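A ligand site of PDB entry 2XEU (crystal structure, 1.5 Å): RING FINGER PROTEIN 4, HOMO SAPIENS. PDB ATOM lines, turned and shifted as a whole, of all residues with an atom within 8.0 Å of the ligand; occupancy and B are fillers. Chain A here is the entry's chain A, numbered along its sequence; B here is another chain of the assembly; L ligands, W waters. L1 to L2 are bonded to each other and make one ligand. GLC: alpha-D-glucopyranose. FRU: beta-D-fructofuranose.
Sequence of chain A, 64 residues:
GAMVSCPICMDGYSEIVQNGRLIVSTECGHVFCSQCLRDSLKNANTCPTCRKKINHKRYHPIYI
OXT of Ile 64 lies within hydrogen-bond range of O4 of FRU L2, at 2.8 Å. O6 of FRU L2 sits at hydrogen-bond distance from O of Arg 21, 3.0 Å away. The backbone NH (N) of Ile 64 sits at hydrogen-bond distance from an oxygen (O4) of FRU L2, 3.2 Å away.
The backbone NH (N) of Ile 62 sits at hydrogen-bond distance from the backbone carbonyl oxygen (O) of Ile 23 (2.9 Å). The side-chain hydroxyl (OH) of Tyr 13 is in hydrogen-bond range of the chain-end carboxylate (OXT) of Ile 64 (2.6 Å). O of Gly 29 of chain B is in hydrogen-bond range of N of Tyr 63, at 2.8 Å. The backbone NH (N) of Arg 21 is in hydrogen-bond range of the backbone carbonyl oxygen (O) of Ile 16 (3.2 Å). O of Leu 22 sits at hydrogen-bond distance from N of Ser 34, at 2.9 Å. The guanidinium group (NE) of Arg 21 sits at hydrogen-bond distance from the side-chain amide oxygen (OD1) of Asn 19, at 3.2 Å. N of Gly 1 lies within hydrogen-bond range of O of Ile 64, at 3.0 Å.
OH of Tyr 13 touches O1 of FRU L2 (3.5 Å). CG1 of Val 17 touches O6 of FRU L2 (3.4 Å). CD2 of Leu 22 touches C6 of GLC L1 (3.5 Å). Ile 62 touches the ligand. CB of Tyr 63 touches O3 of FRU L2 (3.6 Å). Within 4 Å of the ligand: Tyr 13, Val 17, Arg 21, Leu 22, Ile 62, Tyr 63 and Ile 64.
Water W2 lies within hydrogen-bond range of an oxygen (O1) of FRU L2 (2.5 Å) and the side-chain hydroxyl of Tyr 13 (2.7 Å). Water W1 lies within hydrogen-bond range of an oxygen (O4) of FRU L2 (2.7 Å), the backbone carbonyl oxygen of Ile 62 (2.8 Å) and the backbone NH of Ile 23 (2.8 Å). Water W4 bridges O6 of GLC L1 (2.8 Å) and O of Gly 20 (2.9 Å). Water W8 lies within hydrogen-bond range of OH of Tyr 63 (2.7 Å) and O4 of GLC L1 (3.0 Å).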
ATOM      1  N   GLY A   1      -7.264  17.662  13.449  1.00  0.00           N
ATOM      2  CA  GLY A   1      -8.207  16.531  13.311  1.00  0.00           C
ATOM      3  C   GLY A   1      -7.963  15.733  12.052  1.00  0.00           C
ATOM      4  O   GLY A   1      -7.581  16.273  11.014  1.00  0.00           O
ATOM      5  N   ALA A   2      -8.182  14.435  12.157  1.00  0.00           N
ATOM      6  CA  ALA A   2      -7.986  13.532  11.061  1.00  0.00           C
ATOM      7  C   ALA A   2      -8.887  12.336  11.271  1.00  0.00           C
ATOM      8  O   ALA A   2      -9.460  12.153  12.349  1.00  0.00           O
ATOM      9  CB  ALA A   2      -6.524  13.072  11.007  1.00  0.00           C
ATOM     10  N   TYR A  13      -9.471   7.998  15.223  1.00  0.00           N
ATOM     11  CA  TYR A  13      -8.734   9.164  15.705  1.00  0.00           C
ATOM     12  C   TYR A  13      -9.421   9.836  16.884  1.00  0.00           C
ATOM     13  O   TYR A  13      -8.776  10.141  17.870  1.00  0.00           O
ATOM     14  CB  TYR A  13      -8.599  10.171  14.565  1.00  0.00           C
ATOM     15  CG  TYR A  13      -7.953  11.494  14.930  1.00  0.00           C
ATOM     16  CD1 TYR A  13      -6.590  11.682  14.800  1.00  0.00           C
ATOM     17  CD2 TYR A  13      -8.728  12.555  15.384  1.00  0.00           C
ATOM     18  CE1 TYR A  13      -6.002  12.899  15.109  1.00  0.00           C
ATOM     19  CE2 TYR A  13      -8.158  13.763  15.713  1.00  0.00           C
ATOM     20  CZ  TYR A  13      -6.795  13.935  15.576  1.00  0.00           C
ATOM     21  OH  TYR A  13      -6.248  15.163  15.874  1.00  0.00           O
ATOM     22  N   ILE A  16      -8.878   7.866  20.028  1.00  0.00           N
ATOM     23  CA  ILE A  16      -7.462   7.880  20.400  1.00  0.00           C
ATOM     24  C   ILE A  16      -7.096   9.196  21.096  1.00  0.00           C
ATOM     25  O   ILE A  16      -6.505   9.196  22.170  1.00  0.00           O
ATOM     26  CB  ILE A  16      -6.561   7.683  19.167  1.00  0.00           C
ATOM     27  CG1 ILE A  16      -6.713   6.260  18.611  1.00  0.00           C
ATOM     28  CG2 ILE A  16      -5.104   7.934  19.493  1.00  0.00           C
ATOM     29  CD1 ILE A  16      -6.157   6.107  17.215  1.00  0.00           C
ATOM     30  N   VAL A  17      -7.445  10.307  20.466  1.00  0.00           N
ATOM     31  CA  VAL A  17      -7.081  11.603  21.014  1.00  0.00           C
ATOM     32  C   VAL A  17      -7.951  11.979  22.237  1.00  0.00           C
ATOM     33  O   VAL A  17      -7.468  12.659  23.130  1.00  0.00           O
ATOM     34  CB  VAL A  17      -7.088  12.733  19.934  1.00  0.00           C
ATOM     35  CG1 VAL A  17      -6.157  12.356  18.784  1.00  0.00           C
ATOM     36  CG2 VAL A  17      -8.496  13.009  19.437  1.00  0.00           C
ATOM     37  N   GLN A  18      -9.189  11.504  22.285  1.00  0.00           N
ATOM     38  CA  GLN A  18     -10.061  11.714  23.471  1.00  0.00           C
ATOM     39  C   GLN A  18      -9.419  11.140  24.746  1.00  0.00           C
ATOM     40  O   GLN A  18      -9.633  11.667  25.845  1.00  0.00           O
ATOM     41  CB  GLN A  18     -11.447  11.085  23.266  1.00  0.00           C
ATOM     42  CG  GLN A  18     -12.428  11.251  24.444  1.00  0.00           C
ATOM     43  CD  GLN A  18     -13.632  10.304  24.374  1.00  0.00           C
ATOM     44  OE1 GLN A  18     -13.579   9.235  23.755  1.00  0.00           O
ATOM     45  NE2 GLN A  18     -14.730  10.700  25.025  1.00  0.00           N
ATOM     46  N   ASN A  19      -8.681  10.054  24.567  1.00  0.00           N
ATOM     47  CA  ASN A  19      -8.014   9.306  25.627  1.00  0.00           C
ATOM     48  C   ASN A  19      -6.581   9.787  25.914  1.00  0.00           C
ATOM     49  O   ASN A  19      -5.823   9.113  26.600  1.00  0.00           O
ATOM     50  CB  ASN A  19      -7.994   7.827  25.182  1.00  0.00           C
ATOM     51  CG  ASN A  19      -7.715   6.858  26.312  1.00  0.00           C
ATOM     52  OD1 ASN A  19      -6.808   6.025  26.206  1.00  0.00           O
ATOM     53  ND2 ASN A  19      -8.493   6.945  27.383  1.00  0.00           N
ATOM     54  N   GLY A  20      -6.170  10.923  25.350  1.00  0.00           N
ATOM     55  CA  GLY A  20      -4.828  11.462  25.608  1.00  0.00           C
ATOM     56  C   GLY A  20      -3.656  10.764  24.913  1.00  0.00           C
ATOM     57  O   GLY A  20      -2.487  11.012  25.247  1.00  0.00           O
ATOM     58  N   ARG A  21      -3.961   9.886  23.962  1.00  0.00           N
ATOM     59  CA  ARG A  21      -2.923   9.201  23.211  1.00  0.00           C
ATOM     60  C   ARG A  21      -2.486  10.061  22.035  1.00  0.00           C
ATOM     61  O   ARG A  21      -3.184  10.988  21.622  1.00  0.00           O
ATOM     62  CB  ARG A  21      -3.413   7.832  22.739  1.00  0.00           C
ATOM     63  CG  ARG A  21      -3.489   6.797  23.852  1.00  0.00           C
ATOM     64  CD  ARG A  21      -4.152   5.510  23.386  1.00  0.00           C
ATOM     65  NE  ARG A  21      -5.592   5.662  23.218  1.00  0.00           N
ATOM     66  CZ  ARG A  21      -6.374   4.815  22.545  1.00  0.00           C
ATOM     67  NH1 ARG A  21      -5.878   3.744  21.937  1.00  0.00           N
ATOM     68  NH2 ARG A  21      -7.682   5.054  22.460  1.00  0.00           N
ATOM     69  N   LEU A  22      -1.295   9.752  21.531  1.00  0.00           N
ATOM     70  CA  LEU A  22      -0.774  10.377  20.327  1.00  0.00           C
ATOM     71  C   LEU A  22      -0.975   9.456  19.144  1.00  0.00           C
ATOM     72  O   LEU A  22      -1.031   8.236  19.309  1.00  0.00           O
ATOM     73  CB  LEU A  22       0.728  10.653  20.474  1.00  0.00           C
ATOM     74  CG  LEU A  22       1.146  11.658  21.548  1.00  0.00           C
ATOM     75  CD1 LEU A  22       2.630  11.530  21.865  1.00  0.00           C
ATOM     76  CD2 LEU A  22       0.825  13.060  21.089  1.00  0.00           C
ATOM     77  N   ILE A  23      -1.078  10.029  17.964  1.00  0.00           N
ATOM     78  CA  ILE A  23      -0.917   9.255  16.739  1.00  0.00           C
ATOM     79  C   ILE A  23       0.595   9.214  16.492  1.00  0.00           C
ATOM     80  O   ILE A  23       1.266  10.237  16.571  1.00  0.00           O
ATOM     81  CB  ILE A  23      -1.636   9.888  15.536  1.00  0.00           C
ATOM     82  CG1 ILE A  23      -3.095  10.246  15.849  1.00  0.00           C
ATOM     83  CG2 ILE A  23      -1.571   8.944  14.335  1.00  0.00           C
ATOM     84  CD1 ILE A  23      -3.956   9.096  16.202  1.00  0.00           C
ATOM     85  N   VAL A  24       1.125   8.034  16.217  1.00  0.00           N
ATOM     86  CA  VAL A  24       2.556   7.875  15.968  1.00  0.00           C
ATOM     87  C   VAL A  24       2.792   7.112  14.686  1.00  0.00           C
ATOM     88  O   VAL A  24       1.947   6.342  14.236  1.00  0.00           O
ATOM     89  CB  VAL A  24       3.267   7.159  17.131  1.00  0.00           C
ATOM     90  CG1 VAL A  24       3.056   7.935  18.441  1.00  0.00           C
ATOM     91  CG2 VAL A  24       2.799   5.721  17.285  1.00  0.00           C
ATOM     92  N   SER A  34      -0.107   5.707  20.273  1.00  0.00           N
ATOM     93  CA  SER A  34       1.097   5.615  21.087  1.00  0.00           C
ATOM     94  C   SER A  34       1.092   4.471  22.100  1.00  0.00           C
ATOM     95  O   SER A  34       2.115   3.841  22.338  1.00  0.00           O
ATOM     96  CB  SER A  34       1.355   6.943  21.790  1.00  0.00           C
ATOM     97  OG  SER A  34       0.199   7.414  22.488  1.00  0.00           O
ATOM     98  N   PRO A  61       5.740  10.980  17.061  1.00  0.00           N
ATOM     99  CA  PRO A  61       4.370  11.430  16.836  1.00  0.00           C
ATOM    100  C   PRO A  61       4.176  11.994  15.442  1.00  0.00           C
ATOM    101  O   PRO A  61       5.139  12.489  14.809  1.00  0.00           O
ATOM    102  CB  PRO A  61       4.192  12.536  17.881  1.00  0.00           C
ATOM    103  CG  PRO A  61       5.257  12.350  18.850  1.00  0.00           C
ATOM    104  CD  PRO A  61       6.404  11.734  18.126  1.00  0.00           C
ATOM    105  N   ILE A  62       2.944  11.924  14.955  1.00  0.00           N
ATOM    106  CA  ILE A  62       2.516  12.688  13.798  1.00  0.00           C
ATOM    107  C   ILE A  62       1.336  13.580  14.227  1.00  0.00           C
ATOM    108  O   ILE A  62       0.357  13.122  14.801  1.00  0.00           O
ATOM    109  CB  ILE A  62       2.177  11.818  12.561  1.00  0.00           C
ATOM    110  CG1 ILE A  62       1.057  10.802  12.846  1.00  0.00           C
ATOM    111  CG2 ILE A  62       3.429  11.107  12.041  1.00  0.00           C
ATOM    112  CD1 ILE A  62       0.609  10.076  11.600  1.00  0.00           C
ATOM    113  N   TYR A  63       1.478  14.861  13.956  1.00  0.00           N
ATOM    114  CA  TYR A  63       0.570  15.851  14.450  1.00  0.00           C
ATOM    115  C   TYR A  63      -0.492  16.123  13.410  1.00  0.00           C
ATOM    116  O   TYR A  63      -0.346  16.993  12.551  1.00  0.00           O
ATOM    117  CB  TYR A  63       1.338  17.107  14.819  1.00  0.00           C
ATOM    118  CG  TYR A  63       2.319  16.846  15.928  1.00  0.00           C
ATOM    119  CD1 TYR A  63       1.866  16.560  17.201  1.00  0.00           C
ATOM    120  CD2 TYR A  63       3.688  16.855  15.702  1.00  0.00           C
ATOM    121  CE1 TYR A  63       2.745  16.295  18.219  1.00  0.00           C
ATOM    122  CE2 TYR A  63       4.581  16.605  16.729  1.00  0.00           C
ATOM    123  CZ  TYR A  63       4.096  16.327  17.985  1.00  0.00           C
ATOM    124  OH  TYR A  63       4.963  16.057  19.031  1.00  0.00           O
ATOM    125  N   ILE A  64      -1.570  15.357  13.514  1.00  0.00           N
ATOM    126  CA  ILE A  64      -2.682  15.458  12.569  1.00  0.00           C
ATOM    127  C   ILE A  64      -3.992  15.622  13.305  1.00  0.00           C
ATOM    128  O   ILE A  64      -5.025  15.870  12.677  1.00  0.00           O
ATOM    129  CB  ILE A  64      -2.753  14.221  11.625  1.00  0.00           C
ATOM    130  CG1 ILE A  64      -2.981  12.911  12.402  1.00  0.00           C
ATOM    131  CG2 ILE A  64      -1.490  14.149  10.776  1.00  0.00           C
ATOM    132  CD1 ILE A  64      -3.125  11.680  11.523  1.00  0.00           C
ATOM    133  OXT ILE A  64      -4.062  15.540  14.535  1.00  0.00           O
ATOM    134  N   GLY B  29       7.172  15.253  12.922  1.00  0.00           N
ATOM    135  CA  GLY B  29       5.768  14.904  12.991  1.00  0.00           C
ATOM    136  C   GLY B  29       4.825  15.721  12.137  1.00  0.00           C
ATOM    137  O   GLY B  29       3.609  15.690  12.333  1.00  0.00           O
ATOM    138  N   HIS B  30       5.363  16.454  11.169  1.00  0.00           N
ATOM    139  CA  HIS B  30       4.559  17.313  10.326  1.00  0.00           C
ATOM    140  C   HIS B  30       4.274  16.654   8.986  1.00  0.00           C
ATOM    141  O   HIS B  30       5.196  16.167   8.309  1.00  0.00           O
ATOM    142  CB  HIS B  30       5.200  18.687  10.272  1.00  0.00           C
ATOM    143  CG  HIS B  30       5.238  19.323  11.620  1.00  0.00           C
ATOM    144  ND1 HIS B  30       6.401  19.747  12.237  1.00  0.00           N
ATOM    145  CD2 HIS B  30       4.252  19.481  12.534  1.00  0.00           C
ATOM    146  CE1 HIS B  30       6.104  20.182  13.452  1.00  0.00           C
ATOM    147  NE2 HIS B  30       4.804  20.026  13.653  1.00  0.00           N
HETATM  148  C1  GLC L   1      -2.118  18.424  20.590  1.00  0.00           C
HETATM  149  C2  GLC L   1      -1.045  19.469  20.820  1.00  0.00           C
HETATM  150  C3  GLC L   1       0.337  18.817  20.856  1.00  0.00           C
HETATM  151  C4  GLC L   1       0.366  17.689  21.886  1.00  0.00           C
HETATM  152  C5  GLC L   1      -0.762  16.704  21.621  1.00  0.00           C
HETATM  153  C6  GLC L   1      -0.873  15.636  22.709  1.00  0.00           C
HETATM  154  O2  GLC L   1      -1.124  20.465  19.811  1.00  0.00           O
HETATM  155  O3  GLC L   1       1.320  19.782  21.161  1.00  0.00           O
HETATM  156  O4  GLC L   1       1.589  17.000  21.854  1.00  0.00           O
HETATM  157  O5  GLC L   1      -1.991  17.372  21.540  1.00  0.00           O
HETATM  158  O6  GLC L   1      -1.187  16.197  23.969  1.00  0.00           O
HETATM  159  C1  FRU L   2      -4.232  18.455  18.492  1.00  0.00           C
HETATM  160  C2  FRU L   2      -3.150  17.405  18.625  1.00  0.00           C
HETATM  161  C3  FRU L   2      -2.741  16.847  17.262  1.00  0.00           C
HETATM  162  C4  FRU L   2      -2.322  15.442  17.649  1.00  0.00           C
HETATM  163  C5  FRU L   2      -3.335  15.098  18.744  1.00  0.00           C
HETATM  164  C6  FRU L   2      -2.765  14.116  19.743  1.00  0.00           C
HETATM  165  O1  FRU L   2      -5.365  17.942  17.817  1.00  0.00           O
HETATM  166  O2  FRU L   2      -1.989  17.930  19.269  1.00  0.00           O
HETATM  167  O3  FRU L   2      -1.724  17.595  16.650  1.00  0.00           O
HETATM  168  O4  FRU L   2      -2.341  14.555  16.555  1.00  0.00           O
HETATM  169  O5  FRU L   2      -3.663  16.319  19.374  1.00  0.00           O
HETATM  170  O6  FRU L   2      -3.732  13.799  20.741  1.00  0.00           O
HETATM  171  O   HOH W   1      -0.480  12.725  17.419  1.00  0.00           O
HETATM  172  O   HOH W   2      -7.434  16.604  17.845  1.00  0.00           O
HETATM  173  O   HOH W   3       1.029  16.178  25.827  1.00  0.00           O
HETATM  174  O   HOH W   4      -1.335  13.691  25.161  1.00  0.00           O
HETATM  175  O   HOH W   5       2.953  19.893  18.290  1.00  0.00           O
HETATM  176  O   HOH W   6       0.232  19.758  17.365  1.00  0.00           O
HETATM  177  O   HOH W   7       1.842  22.666  19.514  1.00  0.00           O
HETATM  178  O   HOH W   8       4.141  18.116  20.644  1.00  0.00           O
